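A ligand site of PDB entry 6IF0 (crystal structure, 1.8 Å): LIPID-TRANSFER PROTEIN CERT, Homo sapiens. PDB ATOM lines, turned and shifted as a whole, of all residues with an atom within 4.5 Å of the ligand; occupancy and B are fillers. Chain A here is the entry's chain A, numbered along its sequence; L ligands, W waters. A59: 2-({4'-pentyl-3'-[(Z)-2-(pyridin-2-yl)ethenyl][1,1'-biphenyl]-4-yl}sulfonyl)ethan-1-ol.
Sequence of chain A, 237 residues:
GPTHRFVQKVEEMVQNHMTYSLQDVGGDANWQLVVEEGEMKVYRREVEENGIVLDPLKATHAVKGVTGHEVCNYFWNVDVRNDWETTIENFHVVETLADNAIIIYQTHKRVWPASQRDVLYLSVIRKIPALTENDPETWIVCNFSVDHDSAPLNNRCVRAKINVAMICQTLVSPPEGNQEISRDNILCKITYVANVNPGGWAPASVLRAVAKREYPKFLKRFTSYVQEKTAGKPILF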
ATOM      1  N   PHE A  75     -20.103  -6.345  35.525  1.00  0.00           N
ATOM      2  CA  PHE A  75     -19.997  -7.312  34.450  1.00  0.00           C
ATOM      3  C   PHE A  75     -20.017  -6.579  33.110  1.00  0.00           C
ATOM      4  O   PHE A  75     -19.336  -6.940  32.151  1.00  0.00           O
ATOM      5  CB  PHE A  75     -21.062  -8.412  34.612  1.00  0.00           C
ATOM      6  CG  PHE A  75     -20.961  -9.539  33.606  1.00  0.00           C
ATOM      7  CD1 PHE A  75     -19.848 -10.367  33.558  1.00  0.00           C
ATOM      8  CD2 PHE A  75     -21.998  -9.804  32.722  1.00  0.00           C
ATOM      9  CE1 PHE A  75     -19.792 -11.423  32.664  1.00  0.00           C
ATOM     10  CE2 PHE A  75     -21.937 -10.856  31.821  1.00  0.00           C
ATOM     11  CZ  PHE A  75     -20.829 -11.679  31.785  1.00  0.00           C
ATOM     12  N   ARG A  81     -13.177  -4.277  32.682  1.00  0.00           N
ATOM     13  CA  ARG A  81     -13.123  -5.612  32.105  1.00  0.00           C
ATOM     14  C   ARG A  81     -11.774  -6.268  32.421  1.00  0.00           C
ATOM     15  O   ARG A  81     -11.730  -7.392  32.910  1.00  0.00           O
ATOM     16  CB  ARG A  81     -13.398  -5.515  30.601  1.00  0.00           C
ATOM     17  CG  ARG A  81     -13.600  -6.863  29.936  1.00  0.00           C
ATOM     18  CD  ARG A  81     -14.921  -7.527  30.350  1.00  0.00           C
ATOM     19  NE  ARG A  81     -15.803  -7.631  29.196  1.00  0.00           N
ATOM     20  CZ  ARG A  81     -16.921  -6.943  29.031  1.00  0.00           C
ATOM     21  NH1 ARG A  81     -17.581  -7.064  27.898  1.00  0.00           N
ATOM     22  NH2 ARG A  81     -17.361  -6.135  29.983  1.00  0.00           N
ATOM     23  N   TRP A  84     -10.867  -8.128  35.822  1.00  0.00           N
ATOM     24  CA  TRP A  84     -11.349  -9.419  36.305  1.00  0.00           C
ATOM     25  C   TRP A  84     -11.189 -10.528  35.254  1.00  0.00           C
ATOM     26  O   TRP A  84     -11.131 -11.709  35.608  1.00  0.00           O
ATOM     27  CB  TRP A  84     -12.808  -9.364  36.824  1.00  0.00           C
ATOM     28  CG  TRP A  84     -13.812  -8.835  35.838  1.00  0.00           C
ATOM     29  CD1 TRP A  84     -14.296  -7.563  35.771  1.00  0.00           C
ATOM     30  CD2 TRP A  84     -14.512  -9.592  34.837  1.00  0.00           C
ATOM     31  NE1 TRP A  84     -15.226  -7.463  34.759  1.00  0.00           N
ATOM     32  CE2 TRP A  84     -15.393  -8.695  34.176  1.00  0.00           C
ATOM     33  CE3 TRP A  84     -14.490 -10.926  34.427  1.00  0.00           C
ATOM     34  CZ2 TRP A  84     -16.203  -9.093  33.120  1.00  0.00           C
ATOM     35  CZ3 TRP A  84     -15.292 -11.326  33.376  1.00  0.00           C
ATOM     36  CH2 TRP A  84     -16.133 -10.417  32.735  1.00  0.00           C
ATOM     37  N   GLU A  85     -11.148 -10.142  33.985  1.00  0.00           N
ATOM     38  CA  GLU A  85     -11.082 -11.085  32.887  1.00  0.00           C
ATOM     39  C   GLU A  85      -9.683 -11.666  32.894  1.00  0.00           C
ATOM     40  O   GLU A  85      -8.737 -10.911  33.094  1.00  0.00           O
ATOM     41  CB  GLU A  85     -11.123 -10.360  31.541  1.00  0.00           C
ATOM     42  CG  GLU A  85     -12.527 -10.041  31.083  1.00  0.00           C
ATOM     43  CD  GLU A  85     -13.198 -11.158  30.286  1.00  0.00           C
ATOM     44  OE1 GLU A  85     -13.982 -10.824  29.379  1.00  0.00           O
ATOM     45  OE2 GLU A  85     -12.922 -12.359  30.549  1.00  0.00           O
ATOM     46  N   THR A  87      -9.096 -14.419  30.416  1.00  0.00           N
ATOM     47  CA  THR A  87      -8.976 -15.250  29.236  1.00  0.00           C
ATOM     48  C   THR A  87      -8.985 -14.420  27.950  1.00  0.00           C
ATOM     49  O   THR A  87      -8.960 -14.979  26.858  1.00  0.00           O
ATOM     50  CB  THR A  87     -10.083 -16.317  29.190  1.00  0.00           C
ATOM     51  OG1 THR A  87     -11.338 -15.640  29.094  1.00  0.00           O
ATOM     52  CG2 THR A  87     -10.085 -17.205  30.419  1.00  0.00           C
ATOM     53  N   ILE A  88      -8.984 -13.094  28.087  1.00  0.00           N
ATOM     54  CA  ILE A  88      -9.111 -12.194  26.947  1.00  0.00           C
ATOM     55  C   ILE A  88      -7.706 -11.772  26.512  1.00  0.00           C
ATOM     56  O   ILE A  88      -6.897 -11.400  27.361  1.00  0.00           O
ATOM     57  CB  ILE A  88      -9.894 -10.957  27.435  1.00  0.00           C
ATOM     58  CG1 ILE A  88     -11.366 -11.296  27.695  1.00  0.00           C
ATOM     59  CG2 ILE A  88      -9.758  -9.789  26.484  1.00  0.00           C
ATOM     60  CD1 ILE A  88     -12.041 -11.929  26.534  1.00  0.00           C
ATOM     61  N   GLN A 106     -13.748  -9.296  20.620  1.00  0.00           N
ATOM     62  CA  GLN A 106     -12.658  -9.687  21.520  1.00  0.00           C
ATOM     63  C   GLN A 106     -12.031 -10.986  21.069  1.00  0.00           C
ATOM     64  O   GLN A 106     -12.693 -11.795  20.420  1.00  0.00           O
ATOM     65  CB  GLN A 106     -13.044  -9.820  22.991  1.00  0.00           C
ATOM     66  CG  GLN A 106     -14.005 -10.982  23.258  1.00  0.00           C
ATOM     67  CD  GLN A 106     -14.650 -10.896  24.626  1.00  0.00           C
ATOM     68  OE1 GLN A 106     -15.037  -9.815  25.102  1.00  0.00           O
ATOM     69  NE2 GLN A 106     -14.909 -12.046  25.218  1.00  0.00           N
ATOM     70  N   HIS A 108      -9.831 -14.377  22.449  1.00  0.00           N
ATOM     71  CA  HIS A 108      -9.514 -15.175  23.625  1.00  0.00           C
ATOM     72  C   HIS A 108      -8.079 -15.704  23.606  1.00  0.00           C
ATOM     73  O   HIS A 108      -7.549 -16.044  22.567  1.00  0.00           O
ATOM     74  CB  HIS A 108     -10.599 -16.231  23.829  1.00  0.00           C
ATOM     75  CG  HIS A 108     -11.807 -15.579  24.402  1.00  0.00           C
ATOM     76  ND1 HIS A 108     -11.954 -15.348  25.772  1.00  0.00           N
ATOM     77  CD2 HIS A 108     -12.900 -15.038  23.811  1.00  0.00           C
ATOM     78  CE1 HIS A 108     -13.127 -14.759  25.992  1.00  0.00           C
ATOM     79  NE2 HIS A 108     -13.718 -14.545  24.796  1.00  0.00           N
ATOM     80  N   VAL A 111      -5.904 -21.593  23.604  1.00  0.00           N
ATOM     81  CA  VAL A 111      -5.824 -22.747  24.485  1.00  0.00           C
ATOM     82  C   VAL A 111      -5.219 -23.916  23.688  1.00  0.00           C
ATOM     83  O   VAL A 111      -5.900 -24.527  22.872  1.00  0.00           O
ATOM     84  CB  VAL A 111      -7.217 -23.043  25.062  1.00  0.00           C
ATOM     85  CG1 VAL A 111      -7.310 -24.421  25.706  1.00  0.00           C
ATOM     86  CG2 VAL A 111      -7.604 -21.964  26.073  1.00  0.00           C
ATOM     87  N   ALA A 114      -5.829 -25.935  20.434  1.00  0.00           N
ATOM     88  CA  ALA A 114      -6.867 -25.438  19.554  1.00  0.00           C
ATOM     89  C   ALA A 114      -6.439 -24.068  19.035  1.00  0.00           C
ATOM     90  O   ALA A 114      -5.617 -23.387  19.634  1.00  0.00           O
ATOM     91  CB  ALA A 114      -8.163 -25.371  20.290  1.00  0.00           C
ATOM     92  N   SER A 115      -6.974 -23.699  17.877  1.00  0.00           N
ATOM     93  CA  SER A 115      -6.679 -22.368  17.356  1.00  0.00           C
ATOM     94  C   SER A 115      -7.457 -21.329  18.164  1.00  0.00           C
ATOM     95  O   SER A 115      -8.399 -21.650  18.899  1.00  0.00           O
ATOM     96  CB  SER A 115      -6.886 -22.319  15.876  1.00  0.00           C
ATOM     97  OG  SER A 115      -8.256 -22.289  15.603  1.00  0.00           O
ATOM     98  N   ARG A 117      -9.858 -18.381  19.392  1.00  0.00           N
ATOM     99  CA  ARG A 117     -11.202 -17.972  19.002  1.00  0.00           C
ATOM    100  C   ARG A 117     -11.343 -16.452  19.160  1.00  0.00           C
ATOM    101  O   ARG A 117     -10.763 -15.872  20.080  1.00  0.00           O
ATOM    102  CB  ARG A 117     -12.229 -18.673  19.910  1.00  0.00           C
ATOM    103  CG  ARG A 117     -12.886 -19.889  19.273  1.00  0.00           C
ATOM    104  CD  ARG A 117     -11.844 -20.997  19.029  1.00  0.00           C
ATOM    105  NE  ARG A 117     -12.479 -22.130  18.391  1.00  0.00           N
ATOM    106  CZ  ARG A 117     -11.822 -23.123  17.846  1.00  0.00           C
ATOM    107  NH1 ARG A 117     -10.491 -23.184  17.940  1.00  0.00           N
ATOM    108  NH2 ARG A 117     -12.486 -24.013  17.157  1.00  0.00           N
ATOM    109  N   VAL A 119     -14.732 -13.353  19.064  1.00  0.00           N
ATOM    110  CA  VAL A 119     -16.159 -13.230  19.284  1.00  0.00           C
ATOM    111  C   VAL A 119     -16.555 -11.813  18.910  1.00  0.00           C
ATOM    112  O   VAL A 119     -15.778 -10.870  19.139  1.00  0.00           O
ATOM    113  CB  VAL A 119     -16.487 -13.456  20.772  1.00  0.00           C
ATOM    114  CG1 VAL A 119     -17.970 -13.770  20.973  1.00  0.00           C
ATOM    115  CG2 VAL A 119     -15.621 -14.539  21.412  1.00  0.00           C
ATOM    116  N   TYR A 121     -20.045  -9.535  19.660  1.00  0.00           N
ATOM    117  CA  TYR A 121     -21.323  -9.687  20.334  1.00  0.00           C
ATOM    118  C   TYR A 121     -21.870  -8.330  20.792  1.00  0.00           C
ATOM    119  O   TYR A 121     -21.104  -7.416  21.103  1.00  0.00           O
ATOM    120  CB  TYR A 121     -21.202 -10.628  21.538  1.00  0.00           C
ATOM    121  CG  TYR A 121     -20.222 -10.188  22.592  1.00  0.00           C
ATOM    122  CD1 TYR A 121     -18.863 -10.445  22.472  1.00  0.00           C
ATOM    123  CD2 TYR A 121     -20.657  -9.566  23.750  1.00  0.00           C
ATOM    124  CE1 TYR A 121     -17.974 -10.047  23.455  1.00  0.00           C
ATOM    125  CE2 TYR A 121     -19.782  -9.182  24.756  1.00  0.00           C
ATOM    126  CZ  TYR A 121     -18.427  -9.449  24.613  1.00  0.00           C
ATOM    127  OH  TYR A 121     -17.551  -9.050  25.576  1.00  0.00           O
ATOM    128  N   ASN A 143     -25.118 -10.986  26.628  1.00  0.00           N
ATOM    129  CA  ASN A 143     -24.071 -10.872  25.624  1.00  0.00           C
ATOM    130  C   ASN A 143     -24.389 -11.911  24.548  1.00  0.00           C
ATOM    131  O   ASN A 143     -24.334 -13.104  24.826  1.00  0.00           O
ATOM    132  CB  ASN A 143     -22.705 -11.178  26.268  1.00  0.00           C
ATOM    133  CG  ASN A 143     -22.327 -10.130  27.295  1.00  0.00           C
ATOM    134  OD1 ASN A 143     -22.700  -8.977  27.141  1.00  0.00           O
ATOM    135  ND2 ASN A 143     -21.569 -10.509  28.330  1.00  0.00           N
ATOM    136  N   ALA A 160     -16.168 -17.645  17.330  1.00  0.00           N
ATOM    137  CA  ALA A 160     -17.130 -18.357  18.165  1.00  0.00           C
ATOM    138  C   ALA A 160     -18.404 -17.534  18.191  1.00  0.00           C
ATOM    139  O   ALA A 160     -18.359 -16.352  17.861  1.00  0.00           O
ATOM    140  CB  ALA A 160     -16.571 -18.423  19.558  1.00  0.00           C
ATOM    141  N   ILE A 162     -21.872 -16.804  20.783  1.00  0.00           N
ATOM    142  CA  ILE A 162     -22.193 -16.940  22.184  1.00  0.00           C
ATOM    143  C   ILE A 162     -23.573 -16.358  22.406  1.00  0.00           C
ATOM    144  O   ILE A 162     -24.047 -15.506  21.648  1.00  0.00           O
ATOM    145  CB  ILE A 162     -21.162 -16.214  23.064  1.00  0.00           C
ATOM    146  CG1 ILE A 162     -21.294 -14.695  22.959  1.00  0.00           C
ATOM    147  CG2 ILE A 162     -19.763 -16.688  22.763  1.00  0.00           C
ATOM    148  CD1 ILE A 162     -20.538 -13.965  24.045  1.00  0.00           C
ATOM    149  N   VAL A 164     -24.852 -15.414  26.272  1.00  0.00           N
ATOM    150  CA  VAL A 164     -24.508 -15.451  27.683  1.00  0.00           C
ATOM    151  C   VAL A 164     -25.483 -14.522  28.391  1.00  0.00           C
ATOM    152  O   VAL A 164     -25.859 -13.496  27.834  1.00  0.00           O
ATOM    153  CB  VAL A 164     -23.058 -14.976  27.886  1.00  0.00           C
ATOM    154  CG1 VAL A 164     -22.747 -14.693  29.347  1.00  0.00           C
ATOM    155  CG2 VAL A 164     -22.068 -16.021  27.327  1.00  0.00           C
ATOM    156  N   TYR A 192     -26.179 -17.551  35.958  1.00  0.00           N
ATOM    157  CA  TYR A 192     -25.305 -17.256  34.842  1.00  0.00           C
ATOM    158  C   TYR A 192     -25.432 -18.403  33.856  1.00  0.00           C
ATOM    159  O   TYR A 192     -25.268 -19.570  34.231  1.00  0.00           O
ATOM    160  CB  TYR A 192     -23.855 -17.119  35.325  1.00  0.00           C
ATOM    161  CG  TYR A 192     -22.840 -16.983  34.209  1.00  0.00           C
ATOM    162  CD1 TYR A 192     -22.559 -15.758  33.611  1.00  0.00           C
ATOM    163  CD2 TYR A 192     -22.196 -18.106  33.719  1.00  0.00           C
ATOM    164  CE1 TYR A 192     -21.658 -15.633  32.564  1.00  0.00           C
ATOM    165  CE2 TYR A 192     -21.295 -17.998  32.661  1.00  0.00           C
ATOM    166  CZ  TYR A 192     -21.020 -16.773  32.101  1.00  0.00           C
ATOM    167  OH  TYR A 192     -20.114 -16.721  31.077  1.00  0.00           O
ATOM    168  N   VAL A 196     -22.156 -21.548  24.105  1.00  0.00           N
ATOM    169  CA  VAL A 196     -21.038 -21.133  23.285  1.00  0.00           C
ATOM    170  C   VAL A 196     -20.863 -22.138  22.162  1.00  0.00           C
ATOM    171  O   VAL A 196     -20.744 -23.349  22.415  1.00  0.00           O
ATOM    172  CB  VAL A 196     -19.733 -20.985  24.087  1.00  0.00           C
ATOM    173  CG1 VAL A 196     -18.560 -20.707  23.146  1.00  0.00           C
ATOM    174  CG2 VAL A 196     -19.879 -19.891  25.123  1.00  0.00           C
ATOM    175  N   PRO A 198     -18.087 -22.909  19.675  1.00  0.00           N
ATOM    176  CA  PRO A 198     -16.690 -22.503  19.493  1.00  0.00           C
ATOM    177  C   PRO A 198     -16.322 -22.340  18.030  1.00  0.00           C
ATOM    178  O   PRO A 198     -15.262 -21.849  17.692  1.00  0.00           O
ATOM    179  CB  PRO A 198     -15.864 -23.640  20.140  1.00  0.00           C
ATOM    180  CG  PRO A 198     -16.794 -24.835  20.178  1.00  0.00           C
ATOM    181  CD  PRO A 198     -18.221 -24.274  20.221  1.00  0.00           C
ATOM    182  N   ALA A 202     -12.602 -28.090  17.525  1.00  0.00           N
ATOM    183  CA  ALA A 202     -11.589 -28.086  18.562  1.00  0.00           C
ATOM    184  C   ALA A 202     -11.759 -29.440  19.241  1.00  0.00           C
ATOM    185  O   ALA A 202     -12.839 -30.017  19.109  1.00  0.00           O
ATOM    186  CB  ALA A 202     -11.778 -26.936  19.527  1.00  0.00           C
ATOM    187  N   LEU A 207     -12.223 -28.516  24.877  1.00  0.00           N
ATOM    188  CA  LEU A 207     -13.336 -27.629  25.151  1.00  0.00           C
ATOM    189  C   LEU A 207     -13.918 -27.947  26.529  1.00  0.00           C
ATOM    190  O   LEU A 207     -14.245 -27.041  27.292  1.00  0.00           O
ATOM    191  CB  LEU A 207     -14.398 -27.837  24.060  1.00  0.00           C
ATOM    192  CG  LEU A 207     -13.980 -27.314  22.685  1.00  0.00           C
ATOM    193  CD1 LEU A 207     -14.992 -27.686  21.614  1.00  0.00           C
ATOM    194  CD2 LEU A 207     -13.817 -25.801  22.720  1.00  0.00           C
ATOM    195  N   VAL A 210     -11.508 -26.775  29.291  1.00  0.00           N
ATOM    196  CA  VAL A 210     -11.528 -25.327  29.440  1.00  0.00           C
ATOM    197  C   VAL A 210     -12.780 -24.920  30.218  1.00  0.00           C
ATOM    198  O   VAL A 210     -12.682 -24.160  31.180  1.00  0.00           O
ATOM    199  CB  VAL A 210     -11.469 -24.626  28.060  1.00  0.00           C
ATOM    200  CG1 VAL A 210     -11.854 -23.139  28.166  1.00  0.00           C
ATOM    201  CG2 VAL A 210     -10.099 -24.799  27.424  1.00  0.00           C
ATOM    202  N   GLU A 214     -12.474 -23.011  33.653  1.00  0.00           N
ATOM    203  CA  GLU A 214     -12.525 -21.572  33.548  1.00  0.00           C
ATOM    204  C   GLU A 214     -13.855 -21.026  34.058  1.00  0.00           C
ATOM    205  O   GLU A 214     -13.885 -19.891  34.523  1.00  0.00           O
ATOM    206  CB  GLU A 214     -12.207 -21.092  32.122  1.00  0.00           C
ATOM    207  CG  GLU A 214     -10.769 -21.333  31.619  1.00  0.00           C
ATOM    208  CD  GLU A 214      -9.631 -20.714  32.430  1.00  0.00           C
ATOM    209  OE1 GLU A 214      -9.864 -19.673  33.111  1.00  0.00           O
ATOM    210  OE2 GLU A 214      -8.527 -21.292  32.415  1.00  0.00           O
ATOM    211  N   TYR A 215     -14.979 -21.757  33.963  1.00  0.00           N
ATOM    212  CA  TYR A 215     -16.219 -21.108  34.407  1.00  0.00           C
ATOM    213  C   TYR A 215     -16.267 -20.885  35.927  1.00  0.00           C
ATOM    214  O   TYR A 215     -16.628 -19.799  36.396  1.00  0.00           O
ATOM    215  CB  TYR A 215     -17.478 -21.816  33.906  1.00  0.00           C
ATOM    216  CG  TYR A 215     -17.807 -21.485  32.478  1.00  0.00           C
ATOM    217  CD1 TYR A 215     -18.164 -20.199  32.071  1.00  0.00           C
ATOM    218  CD2 TYR A 215     -17.767 -22.473  31.510  1.00  0.00           C
ATOM    219  CE1 TYR A 215     -18.482 -19.907  30.744  1.00  0.00           C
ATOM    220  CE2 TYR A 215     -18.059 -22.197  30.190  1.00  0.00           C
ATOM    221  CZ  TYR A 215     -18.443 -20.927  29.809  1.00  0.00           C
ATOM    222  OH  TYR A 215     -18.702 -20.733  28.471  1.00  0.00           O
HETATM  223  C12 A59 L   1     -17.856 -14.327  26.333  1.00  0.00           C
HETATM  224  C13 A59 L   1     -15.229 -21.294  26.084  1.00  0.00           C
HETATM  225  C14 A59 L   1     -14.821 -21.487  27.369  1.00  0.00           C
HETATM  226  C15 A59 L   1     -13.929 -18.547  30.272  1.00  0.00           C
HETATM  227  C17 A59 L   1     -15.145 -20.556  29.652  1.00  0.00           C
HETATM  228  C18 A59 L   1     -14.545 -20.497  28.388  1.00  0.00           C
HETATM  229  C19 A59 L   1     -13.390 -18.555  28.981  1.00  0.00           C
HETATM  230  C20 A59 L   1     -17.821 -12.150  29.474  1.00  0.00           C
HETATM  231  N1  A59 L   1     -13.666 -19.491  28.064  1.00  0.00           N
HETATM  232  C5  A59 L   1     -16.026 -18.899  26.084  1.00  0.00           C
HETATM  233  C6  A59 L   1     -16.176 -17.650  25.407  1.00  0.00           C
HETATM  234  C7  A59 L   1     -18.134 -14.586  27.670  1.00  0.00           C
HETATM  235  C9  A59 L   1     -17.146 -16.761  27.475  1.00  0.00           C
HETATM  236  O2  A59 L   1     -19.880 -12.789  27.808  1.00  0.00           O
HETATM  237  S1  A59 L   1     -18.966 -13.405  28.722  1.00  0.00           S
HETATM  238  O1  A59 L   1     -19.368 -14.148  29.941  1.00  0.00           O
HETATM  239  C21 A59 L   1     -17.155 -11.351  28.349  1.00  0.00           C
HETATM  240  O3  A59 L   1     -15.949 -12.019  27.992  1.00  0.00           O
HETATM  241  C11 A59 L   1     -17.182 -15.315  25.533  1.00  0.00           C
HETATM  242  C10 A59 L   1     -16.832 -16.536  26.138  1.00  0.00           C
HETATM  243  C8  A59 L   1     -17.780 -15.785  28.278  1.00  0.00           C
HETATM  244  C1  A59 L   1     -15.804 -17.488  24.080  1.00  0.00           C
HETATM  245  C23 A59 L   1     -15.217 -18.592  23.406  1.00  0.00           C
HETATM  246  C3  A59 L   1     -15.053 -19.818  24.066  1.00  0.00           C
HETATM  247  C24 A59 L   1     -14.462 -20.993  23.296  1.00  0.00           C
HETATM  248  C25 A59 L   1     -12.954 -21.128  23.481  1.00  0.00           C
HETATM  249  C26 A59 L   1     -12.483 -22.263  22.527  1.00  0.00           C
HETATM  250  C27 A59 L   1     -11.153 -22.770  23.114  1.00  0.00           C
HETATM  251  C28 A59 L   1     -10.500 -23.798  22.168  1.00  0.00           C
HETATM  252  C4  A59 L   1     -15.452 -19.994  25.395  1.00  0.00           C
HETATM  253  C16 A59 L   1     -14.839 -19.577  30.576  1.00  0.00           C
HETATM  254  O   HOH W   1      -7.851 -21.732  21.897  1.00  0.00           O
HETATM  255  O   HOH W   2     -14.678 -13.826  29.119  1.00  0.00           O
HETATM  256  O   HOH W   3     -11.238 -18.993  25.581  1.00  0.00           O
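The side-chain carboxylate (OE1) of Glu 85 lies within hydrogen-bond range of an oxygen (O3) of the ligand (2.7 Å). NE2 of Gln 106 sits at hydrogen-bond distance from O3 of the ligand (3.0 Å). OH of Tyr 192 sits at hydrogen-bond distance from O1 of the ligand (2.9 Å). The side-chain amide nitrogen (ND2) of Asn 143 is in hydrogen-bond range of an oxygen (O2) of the ligand (2.9 Å).
The backbone NH (N) of His 108 lies within hydrogen-bond range of the backbone carbonyl oxygen (O) of Arg 117 (3.0 Å). A ring nitrogen (NE2) of His 108 sits at hydrogen-bond distance from the side-chain amide nitrogen (NE2) of Gln 106 (2.8 Å). The backbone carbonyl oxygen (O) of Thr 87 lies within hydrogen-bond range of a ring nitrogen (ND1) of His 108 (3.2 Å). OH of Tyr 121 lies within hydrogen-bond range of OE1 of Gln 106, 2.7 Å away. The guanidinium group (NE) of Arg 117 sits at hydrogen-bond distance from the backbone carbonyl oxygen (O) of Pro 198 (2.9 Å). O of Asn 143 lies within hydrogen-bond range of N of Val 164, 2.8 Å away. NH1 of Arg 117 sits at hydrogen-bond distance from O of Ser 115, at 2.8 Å. The backbone carbonyl oxygen of Phe 75 is in hydrogen-bond range of the guanidinium group of Arg 81 (3.0 Å).
Residues that only touch the ligand: Tyr 215 (3.3 Å), Ala 114 (3.4 Å), Glu 214 (3.4 Å), Phe 75 (3.4 Å), Val 164 (3.5 Å), Val 210 (3.5 Å), Ile 162 (3.5 Å), Thr 87 (3.6 Å), His 108 (3.6 Å), Tyr 121 (3.6 Å), Val 196 (3.7 Å), Arg 117 (3.8 Å), Leu 207 (3.8 Å) and Val 119 (3.98 Å). Hydrophobic or aromatic side chains within 4 Å of the ligand: Phe 75, His 108, Ala 114, Val 119, Ile 162, Val 164, Tyr 192, Val 196, Leu 207, Val 210 and Tyr 215.
Water W2 lies within hydrogen-bond range of O3 of the ligand and OE2 of Glu 85.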
